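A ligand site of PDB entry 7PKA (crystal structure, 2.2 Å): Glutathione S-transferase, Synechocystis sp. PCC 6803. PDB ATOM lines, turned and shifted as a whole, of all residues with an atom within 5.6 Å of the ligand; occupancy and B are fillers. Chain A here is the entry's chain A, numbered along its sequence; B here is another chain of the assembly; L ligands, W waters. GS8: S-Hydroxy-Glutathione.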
ATOM      1  N   ALA A   7      -5.478  33.527  -3.677  1.00  0.00           N
ATOM      2  CA  ALA A   7      -4.934  34.573  -2.808  1.00  0.00           C
ATOM      3  C   ALA A   7      -5.179  35.905  -3.508  1.00  0.00           C
ATOM      4  O   ALA A   7      -5.419  35.901  -4.714  1.00  0.00           O
ATOM      5  CB  ALA A   7      -3.438  34.339  -2.566  1.00  0.00           C
ATOM      6  N   PRO A   8      -5.170  37.068  -2.807  1.00  0.00           N
ATOM      7  CA  PRO A   8      -5.442  38.336  -3.520  1.00  0.00           C
ATOM      8  C   PRO A   8      -4.470  38.575  -4.673  1.00  0.00           C
ATOM      9  O   PRO A   8      -3.260  38.312  -4.558  1.00  0.00           O
ATOM     10  CB  PRO A   8      -5.378  39.404  -2.417  1.00  0.00           C
ATOM     11  CG  PRO A   8      -5.578  38.641  -1.137  1.00  0.00           C
ATOM     12  CD  PRO A   8      -4.937  37.299  -1.360  1.00  0.00           C
ATOM     13  N   GLN A   9      -5.035  38.956  -5.818  1.00  0.00           N
ATOM     14  CA  GLN A   9      -4.292  39.254  -7.055  1.00  0.00           C
ATOM     15  C   GLN A   9      -3.618  38.018  -7.692  1.00  0.00           C
ATOM     16  O   GLN A   9      -2.820  38.186  -8.621  1.00  0.00           O
ATOM     17  CB  GLN A   9      -3.274  40.397  -6.846  1.00  0.00           C
ATOM     18  CG  GLN A   9      -3.799  41.595  -6.046  1.00  0.00           C
ATOM     19  CD  GLN A   9      -5.003  42.260  -6.681  1.00  0.00           C
ATOM     20  OE1 GLN A   9      -5.084  42.422  -7.905  1.00  0.00           O
ATOM     21  NE2 GLN A   9      -5.962  42.672  -5.863  1.00  0.00           N
ATOM     22  N   SER A  10      -3.929  36.800  -7.212  1.00  0.00           N
ATOM     23  CA  SER A  10      -3.314  35.597  -7.764  1.00  0.00           C
ATOM     24  C   SER A  10      -3.999  35.168  -9.087  1.00  0.00           C
ATOM     25  O   SER A  10      -5.037  35.715  -9.470  1.00  0.00           O
ATOM     26  CB  SER A  10      -3.384  34.469  -6.729  1.00  0.00           C
ATOM     27  OG  SER A  10      -4.611  33.759  -6.771  1.00  0.00           O
ATOM     28  N   ARG A  11      -3.472  34.121  -9.737  1.00  0.00           N
ATOM     29  CA  ARG A  11      -4.075  33.569 -10.935  1.00  0.00           C
ATOM     30  C   ARG A  11      -5.314  32.744 -10.667  1.00  0.00           C
ATOM     31  O   ARG A  11      -5.911  32.284 -11.624  1.00  0.00           O
ATOM     32  CB  ARG A  11      -3.058  32.767 -11.767  1.00  0.00           C
ATOM     33  CG  ARG A  11      -2.098  33.700 -12.438  1.00  0.00           C
ATOM     34  CD  ARG A  11      -0.934  32.965 -13.007  1.00  0.00           C
ATOM     35  NE  ARG A  11      -0.082  33.889 -13.761  1.00  0.00           N
ATOM     36  CZ  ARG A  11       1.105  33.582 -14.256  1.00  0.00           C
ATOM     37  NH1 ARG A  11       1.600  32.365 -14.099  1.00  0.00           N
ATOM     38  NH2 ARG A  11       1.809  34.487 -14.928  1.00  0.00           N
ATOM     39  N   LEU A  33      -0.945  34.195   1.875  1.00  0.00           N
ATOM     40  CA  LEU A  33       0.469  34.162   1.489  1.00  0.00           C
ATOM     41  C   LEU A  33       1.331  35.008   2.407  1.00  0.00           C
ATOM     42  O   LEU A  33       2.425  34.582   2.765  1.00  0.00           O
ATOM     43  CB  LEU A  33       0.673  34.633   0.036  1.00  0.00           C
ATOM     44  CG  LEU A  33      -0.071  33.870  -1.065  1.00  0.00           C
ATOM     45  CD1 LEU A  33       0.388  34.337  -2.435  1.00  0.00           C
ATOM     46  CD2 LEU A  33       0.093  32.360  -0.943  1.00  0.00           C
ATOM     47  N   HIS A  38       0.674  29.029   2.468  1.00  0.00           N
ATOM     48  CA  HIS A  38       0.992  28.228   1.299  1.00  0.00           C
ATOM     49  C   HIS A  38       2.246  27.369   1.535  1.00  0.00           C
ATOM     50  O   HIS A  38       2.390  26.346   0.867  1.00  0.00           O
ATOM     51  CB  HIS A  38       1.168  29.124   0.081  1.00  0.00           C
ATOM     52  CG  HIS A  38       2.271  30.134   0.224  1.00  0.00           C
ATOM     53  ND1 HIS A  38       2.279  31.055   1.272  1.00  0.00           N
ATOM     54  CD2 HIS A  38       3.338  30.363  -0.569  1.00  0.00           C
ATOM     55  CE1 HIS A  38       3.367  31.783   1.080  1.00  0.00           C
ATOM     56  NE2 HIS A  38       4.039  31.395  -0.007  1.00  0.00           N
ATOM     57  N   ARG A  39       3.117  27.728   2.516  1.00  0.00           N
ATOM     58  CA  ARG A  39       4.303  26.927   2.863  1.00  0.00           C
ATOM     59  C   ARG A  39       4.062  25.988   4.070  1.00  0.00           C
ATOM     60  O   ARG A  39       5.026  25.439   4.601  1.00  0.00           O
ATOM     61  CB  ARG A  39       5.506  27.811   3.180  1.00  0.00           C
ATOM     62  CG  ARG A  39       5.767  28.918   2.179  1.00  0.00           C
ATOM     63  CD  ARG A  39       6.307  28.390   0.888  1.00  0.00           C
ATOM     64  NE  ARG A  39       7.550  27.637   1.066  1.00  0.00           N
ATOM     65  CZ  ARG A  39       8.012  26.741   0.178  1.00  0.00           C
ATOM     66  NH1 ARG A  39       7.341  26.508  -0.948  1.00  0.00           N
ATOM     67  NH2 ARG A  39       9.124  26.076   0.424  1.00  0.00           N
ATOM     68  N   GLY A  50       3.991  24.940  -3.231  1.00  0.00           N
ATOM     69  CA  GLY A  50       3.400  26.006  -2.453  1.00  0.00           C
ATOM     70  C   GLY A  50       2.956  27.186  -3.250  1.00  0.00           C
ATOM     71  O   GLY A  50       3.139  28.335  -2.830  1.00  0.00           O
ATOM     72  N   LYS A  51       2.333  26.930  -4.406  1.00  0.00           N
ATOM     73  CA  LYS A  51       1.827  28.022  -5.234  1.00  0.00           C
ATOM     74  C   LYS A  51       0.328  27.917  -5.443  1.00  0.00           C
ATOM     75  O   LYS A  51      -0.221  26.814  -5.508  1.00  0.00           O
ATOM     76  CB  LYS A  51       2.522  28.030  -6.608  1.00  0.00           C
ATOM     77  CG  LYS A  51       4.031  27.897  -6.565  1.00  0.00           C
ATOM     78  CD  LYS A  51       4.698  29.215  -6.782  1.00  0.00           C
ATOM     79  CE  LYS A  51       6.200  29.131  -6.566  1.00  0.00           C
ATOM     80  NZ  LYS A  51       6.813  30.488  -6.675  1.00  0.00           N
ATOM     81  N   VAL A  52      -0.317  29.066  -5.583  1.00  0.00           N
ATOM     82  CA  VAL A  52      -1.721  29.191  -5.920  1.00  0.00           C
ATOM     83  C   VAL A  52      -1.769  29.682  -7.403  1.00  0.00           C
ATOM     84  O   VAL A  52      -0.895  30.416  -7.857  1.00  0.00           O
ATOM     85  CB  VAL A  52      -2.504  30.121  -4.957  1.00  0.00           C
ATOM     86  CG1 VAL A  52      -2.627  29.509  -3.572  1.00  0.00           C
ATOM     87  CG2 VAL A  52      -1.866  31.510  -4.891  1.00  0.00           C
ATOM     88  N   PRO A  53      -2.773  29.246  -8.193  1.00  0.00           N
ATOM     89  CA  PRO A  53      -3.923  28.444  -7.781  1.00  0.00           C
ATOM     90  C   PRO A  53      -3.757  26.915  -7.784  1.00  0.00           C
ATOM     91  O   PRO A  53      -2.779  26.345  -8.288  1.00  0.00           O
ATOM     92  CB  PRO A  53      -4.990  28.881  -8.774  1.00  0.00           C
ATOM     93  CG  PRO A  53      -4.181  29.058 -10.076  1.00  0.00           C
ATOM     94  CD  PRO A  53      -2.887  29.683  -9.598  1.00  0.00           C
ATOM     95  N   TRP A  63      -2.807  21.390  -9.735  1.00  0.00           N
ATOM     96  CA  TRP A  63      -2.199  22.724  -9.653  1.00  0.00           C
ATOM     97  C   TRP A  63      -1.607  23.129 -11.049  1.00  0.00           C
ATOM     98  O   TRP A  63      -1.605  22.314 -11.979  1.00  0.00           O
ATOM     99  CB  TRP A  63      -1.214  22.853  -8.475  1.00  0.00           C
ATOM    100  CG  TRP A  63      -0.278  21.701  -8.338  1.00  0.00           C
ATOM    101  CD1 TRP A  63      -0.476  20.549  -7.627  1.00  0.00           C
ATOM    102  CD2 TRP A  63       1.019  21.577  -8.940  1.00  0.00           C
ATOM    103  NE1 TRP A  63       0.603  19.722  -7.753  1.00  0.00           N
ATOM    104  CE2 TRP A  63       1.548  20.322  -8.557  1.00  0.00           C
ATOM    105  CE3 TRP A  63       1.788  22.397  -9.767  1.00  0.00           C
ATOM    106  CZ2 TRP A  63       2.783  19.866  -9.004  1.00  0.00           C
ATOM    107  CZ3 TRP A  63       3.024  21.949 -10.199  1.00  0.00           C
ATOM    108  CH2 TRP A  63       3.482  20.683  -9.859  1.00  0.00           C
ATOM    109  N   GLU A  64      -1.163  24.389 -11.190  1.00  0.00           N
ATOM    110  CA  GLU A  64      -0.742  25.057 -12.431  1.00  0.00           C
ATOM    111  C   GLU A  64      -2.017  25.576 -13.067  1.00  0.00           C
ATOM    112  O   GLU A  64      -2.883  24.791 -13.472  1.00  0.00           O
ATOM    113  CB  GLU A  64       0.034  24.145 -13.418  1.00  0.00           C
ATOM    114  CG  GLU A  64       1.513  23.978 -13.073  1.00  0.00           C
ATOM    115  CD  GLU A  64       2.289  25.275 -12.999  1.00  0.00           C
ATOM    116  OE1 GLU A  64       2.022  26.193 -13.802  1.00  0.00           O
ATOM    117  OE2 GLU A  64       3.203  25.359 -12.143  1.00  0.00           O
ATOM    118  N   SER A  65      -2.169  26.907 -13.113  1.00  0.00           N
ATOM    119  CA  SER A  65      -3.360  27.577 -13.670  1.00  0.00           C
ATOM    120  C   SER A  65      -3.686  27.092 -15.070  1.00  0.00           C
ATOM    121  O   SER A  65      -4.856  26.871 -15.378  1.00  0.00           O
ATOM    122  CB  SER A  65      -3.162  29.097 -13.671  1.00  0.00           C
ATOM    123  OG  SER A  65      -2.067  29.532 -14.477  1.00  0.00           O
ATOM    124  N   GLY A  66      -2.647  26.842 -15.884  1.00  0.00           N
ATOM    125  CA  GLY A  66      -2.846  26.361 -17.247  1.00  0.00           C
ATOM    126  C   GLY A  66      -3.458  24.979 -17.299  1.00  0.00           C
ATOM    127  O   GLY A  66      -4.390  24.742 -18.066  1.00  0.00           O
ATOM    128  N   ASN A  97       1.361  30.927 -20.618  1.00  0.00           N
ATOM    129  CA  ASN A  97       2.111  30.641 -19.414  1.00  0.00           C
ATOM    130  C   ASN A  97       3.610  30.711 -19.543  1.00  0.00           C
ATOM    131  O   ASN A  97       4.283  30.758 -18.513  1.00  0.00           O
ATOM    132  CB  ASN A  97       1.705  29.283 -18.875  1.00  0.00           C
ATOM    133  CG  ASN A  97       0.399  29.391 -18.113  1.00  0.00           C
ATOM    134  OD1 ASN A  97       0.399  29.730 -16.915  1.00  0.00           O
ATOM    135  ND2 ASN A  97      -0.721  29.155 -18.774  1.00  0.00           N
ATOM    136  N   LEU B  94       3.280  22.056 -17.746  1.00  0.00           N
ATOM    137  CA  LEU B  94       3.160  23.487 -17.453  1.00  0.00           C
ATOM    138  C   LEU B  94       4.140  23.924 -16.398  1.00  0.00           C
ATOM    139  O   LEU B  94       4.708  25.015 -16.496  1.00  0.00           O
ATOM    140  CB  LEU B  94       1.738  23.872 -17.067  1.00  0.00           C
ATOM    141  CG  LEU B  94       0.995  24.244 -18.345  1.00  0.00           C
ATOM    142  CD1 LEU B  94      -0.260  23.582 -18.449  1.00  0.00           C
ATOM    143  CD2 LEU B  94       1.016  25.725 -18.596  1.00  0.00           C
ATOM    144  N   SER B  98       6.983  26.806 -16.957  1.00  0.00           N
ATOM    145  CA  SER B  98       6.773  28.089 -16.310  1.00  0.00           C
ATOM    146  C   SER B  98       7.431  28.123 -14.930  1.00  0.00           C
ATOM    147  O   SER B  98       8.568  28.575 -14.832  1.00  0.00           O
ATOM    148  CB  SER B  98       5.285  28.443 -16.266  1.00  0.00           C
ATOM    149  OG  SER B  98       4.545  27.459 -15.551  1.00  0.00           O
ATOM    150  N   THR B  99       6.748  27.605 -13.875  1.00  0.00           N
ATOM    151  CA  THR B  99       7.249  27.623 -12.489  1.00  0.00           C
ATOM    152  C   THR B  99       8.691  27.166 -12.344  1.00  0.00           C
ATOM    153  O   THR B  99       9.484  27.902 -11.774  1.00  0.00           O
ATOM    154  CB  THR B  99       6.314  26.825 -11.557  1.00  0.00           C
ATOM    155  OG1 THR B  99       4.968  27.221 -11.827  1.00  0.00           O
ATOM    156  CG2 THR B  99       6.654  27.052 -10.100  1.00  0.00           C
ATOM    157  N   LYS B 112      15.791  33.102  -4.438  1.00  0.00           N
ATOM    158  CA  LYS B 112      14.669  32.682  -3.625  1.00  0.00           C
ATOM    159  C   LYS B 112      14.020  31.367  -4.111  1.00  0.00           C
ATOM    160  O   LYS B 112      13.785  30.467  -3.309  1.00  0.00           O
ATOM    161  CB  LYS B 112      13.591  33.781  -3.545  1.00  0.00           C
ATOM    162  CG  LYS B 112      12.491  33.415  -2.536  1.00  0.00           C
ATOM    163  CD  LYS B 112      11.152  33.984  -2.927  1.00  0.00           C
ATOM    164  CE  LYS B 112      10.304  34.280  -1.705  1.00  0.00           C
ATOM    165  NZ  LYS B 112       9.032  34.949  -2.087  1.00  0.00           N
ATOM    166  N   GLU B 113      13.688  31.301  -5.416  1.00  0.00           N
ATOM    167  CA  GLU B 113      12.914  30.197  -5.997  1.00  0.00           C
ATOM    168  C   GLU B 113      13.638  28.900  -6.123  1.00  0.00           C
ATOM    169  O   GLU B 113      13.068  27.861  -5.806  1.00  0.00           O
ATOM    170  CB  GLU B 113      12.341  30.589  -7.366  1.00  0.00           C
ATOM    171  CG  GLU B 113      11.352  31.726  -7.335  1.00  0.00           C
ATOM    172  CD  GLU B 113      10.066  31.344  -6.631  1.00  0.00           C
ATOM    173  OE1 GLU B 113       9.478  30.290  -6.997  1.00  0.00           O
ATOM    174  OE2 GLU B 113       9.650  32.070  -5.701  1.00  0.00           O
ATOM    175  N   ARG B 116      13.989  26.468  -3.098  1.00  0.00           N
ATOM    176  CA  ARG B 116      12.662  25.972  -2.756  1.00  0.00           C
ATOM    177  C   ARG B 116      12.137  24.918  -3.731  1.00  0.00           C
ATOM    178  O   ARG B 116      11.563  23.924  -3.290  1.00  0.00           O
ATOM    179  CB  ARG B 116      11.675  27.133  -2.659  1.00  0.00           C
ATOM    180  CG  ARG B 116      11.865  27.972  -1.422  1.00  0.00           C
ATOM    181  CD  ARG B 116      10.903  29.136  -1.449  1.00  0.00           C
ATOM    182  NE  ARG B 116      10.676  29.666  -0.111  1.00  0.00           N
ATOM    183  CZ  ARG B 116       9.748  30.568   0.197  1.00  0.00           C
ATOM    184  NH1 ARG B 116       8.953  31.065  -0.754  1.00  0.00           N
ATOM    185  NH2 ARG B 116       9.605  30.993   1.446  1.00  0.00           N
HETATM  186  CB1 GS8 L   1       2.536  30.190 -11.235  1.00  0.00           C
HETATM  187  CG1 GS8 L   1       1.847  30.345  -9.894  1.00  0.00           C
HETATM  188  CD1 GS8 L   1       2.419  31.418  -9.003  1.00  0.00           C
HETATM  189  OE1 GS8 L   1       3.522  31.918  -9.196  1.00  0.00           O
HETATM  190  C1  GS8 L   1       0.594  29.024 -12.364  1.00  0.00           C
HETATM  191  O11 GS8 L   1      -0.222  28.417 -11.632  1.00  0.00           O
HETATM  192  O12 GS8 L   1       0.320  29.621 -13.416  1.00  0.00           O
HETATM  193  N1  GS8 L   1       2.859  28.781 -13.245  1.00  0.00           N
HETATM  194  CA1 GS8 L   1       2.076  28.944 -11.999  1.00  0.00           C
HETATM  195  N2  GS8 L   1       1.661  31.768  -7.962  1.00  0.00           N
HETATM  196  CA2 GS8 L   1       2.029  32.770  -6.973  1.00  0.00           C
HETATM  197  CB2 GS8 L   1       0.915  33.798  -6.812  1.00  0.00           C
HETATM  198  SG2 GS8 L   1       1.237  35.082  -5.566  1.00  0.00           S
HETATM  199  O13 GS8 L   1      -0.140  36.004  -5.398  1.00  0.00           O
HETATM  200  C2  GS8 L   1       2.331  32.152  -5.617  1.00  0.00           C
HETATM  201  O2  GS8 L   1       1.625  31.236  -5.203  1.00  0.00           O
HETATM  202  N3  GS8 L   1       3.383  32.634  -4.947  1.00  0.00           N
HETATM  203  CA3 GS8 L   1       3.776  32.113  -3.663  1.00  0.00           C
HETATM  204  C3  GS8 L   1       5.275  31.832  -3.603  1.00  0.00           C
HETATM  205  O32 GS8 L   1       5.905  31.918  -4.674  1.00  0.00           O
HETATM  206  O31 GS8 L   1       5.771  31.551  -2.482  1.00  0.00           O
HETATM  207  O   HOH W   1       0.639  35.002  -9.892  1.00  0.00           O
HETATM  208  O   HOH W   2       6.376  31.009 -10.376  1.00  0.00           O
HETATM  209  O   HOH W   3       0.766  38.813  -6.621  1.00  0.00           O
HETATM  210  O   HOH W   4       8.445  30.235  -3.390  1.00  0.00           O
HETATM  211  O   HOH W   5       5.377  34.533  -6.320  1.00  0.00           O
HETATM  212  O   HOH W   6       1.760  38.247  -4.008  1.00  0.00           O
HETATM  213  O   HOH W   7       0.229  27.202 -15.551  1.00  0.00           O
HETATM  214  O   HOH W   8       2.668  30.394 -15.672  1.00  0.00           O
HETATM  215  O   HOH W   9       6.193  32.957  -8.313  1.00  0.00           O
HETATM  216  O   HOH W  10       5.980  28.756  -2.377  1.00  0.00           O
HETATM  217  O   HOH W  11      -0.309  26.702  -9.505  1.00  0.00           O
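OE1 of Glu 64 lies within salt-bridge range of N1 of the ligand (2.8 Å). The side-chain amino group (NZ) of Lys 51 is in salt-bridge range of an oxygen (O32) of the ligand (2.6 Å). NH1 of Arg 116 of chain B lies within salt-bridge range of O31 of the ligand (3.7 Å). O2 of the ligand is in hydrogen-bond range of N of Val 52, at 2.9 Å. A nitrogen (N2) of the ligand lies within hydrogen-bond range of the backbone carbonyl oxygen of Val 52, 2.9 Å away. The side-chain hydroxyl (OG1) of Thr 99 of chain B lies within hydrogen-bond range of a nitrogen (N1) of the ligand (3.0 Å). NE2 of His 38 is in hydrogen-bond range of O31 of the ligand (3.0 Å). O12 of the ligand lies within hydrogen-bond range of OG of Ser 65, at 2.6 Å. The side-chain hydroxyl (OG) of Ser 98 of chain B lies within hydrogen-bond range of a nitrogen (N1) of the ligand (3.1 Å). The backbone NH (N) of Ser 65 is in hydrogen-bond range of an oxygen (O11) of the ligand (2.9 Å). NH1 of Arg 11 lies within salt-bridge range of O12 of the ligand (3.1 Å).
The side-chain carboxylate (OE1) of Glu 113 of chain B is in salt-bridge range of the side-chain amino group (NZ) of Lys 51, 2.7 Å away. The side-chain hydroxyl of Ser 98 of chain B sits at hydrogen-bond distance from the backbone carbonyl oxygen of Leu 94 of chain B. The side-chain carboxylate (OE2) of Glu 64 sits at hydrogen-bond distance from the side-chain hydroxyl (OG1) of Thr 99 of chain B (2.6 Å). The side-chain hydroxyl (OG) of Ser 10 sits at hydrogen-bond distance from the backbone carbonyl oxygen (O) of Ala 7 (3.1 Å). The side-chain hydroxyl (OG) of Ser 65 sits at hydrogen-bond distance from the side-chain amide oxygen (OD1) of Asn 97. The side-chain carboxylate of Glu 64 is in hydrogen-bond range of the side-chain hydroxyl of Ser 98 of chain B, 3.3 Å away.
Merely in contact with the ligand: Leu 33 (3.3 Å), Asn 97 (3.5 Å), Pro 53 (3.6 Å), Ser 10 (3.8 Å), Glu 113 of chain B (3.9 Å), Gly 50 (3.9 Å) and Pro 8 (3.97 Å). Hydrophobic or aromatic side chains within 4 Å of the ligand: Leu 33, His 38, Val 52 and Pro 53. 16 residues have an atom within 4 Å of the ligand: Pro 8, Ser 10, Arg 11, Leu 33, His 38, Gly 50, Lys 51, Val 52, Pro 53, Glu 64, Ser 65, Asn 97, Ser 98 of chain B, Thr 99 of chain B, Glu 113 of chain B and Arg 116 of chain B. The nearest printed residue that does not touch the ligand is Gln 9 (4.6 Å).
Water W11 lies within hydrogen-bond range of an oxygen (O11) of the ligand (2.7 Å), the backbone carbonyl oxygen of Pro 53 (2.8 Å) and the backbone NH of Glu 64 (3.0 Å). Water W10 lies within hydrogen-bond range of O31 of the ligand (2.8 Å), O of Gly 50 (2.9 Å) and NH1 of Arg 39 (3.0 Å). Water W8 lies within hydrogen-bond range of the side-chain amide oxygen (OD1) of Asn 97 (2.7 Å), the guanidinium group (NH1) of Arg 11 (2.7 Å), a nitrogen (N1) of the ligand (2.9 Å) and the side-chain hydroxyl (OG) of Ser 98 of chain B (3.5 Å). Water W9 bridges an oxygen (OE1) of the ligand (3.0 Å) and the side-chain amino group (NZ) of Lys 51 (3.0 Å). Water W4 lies within hydrogen-bond range of NH1 of Arg 116 of chain B (2.8 Å), O31 of the ligand (3.1 Å) and OE2 of Glu 113 of chain B (3.2 Å). Water W7 lies within hydrogen-bond range of the side-chain carboxylate of Glu 64 (2.7 Å), the side-chain amide oxygen of Asn 97 (2.9 Å), the backbone NH of Gly 66 (2.9 Å), an oxygen (O12) of the ligand (3.2 Å) and the backbone NH of Ser 65 (3.4 Å).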
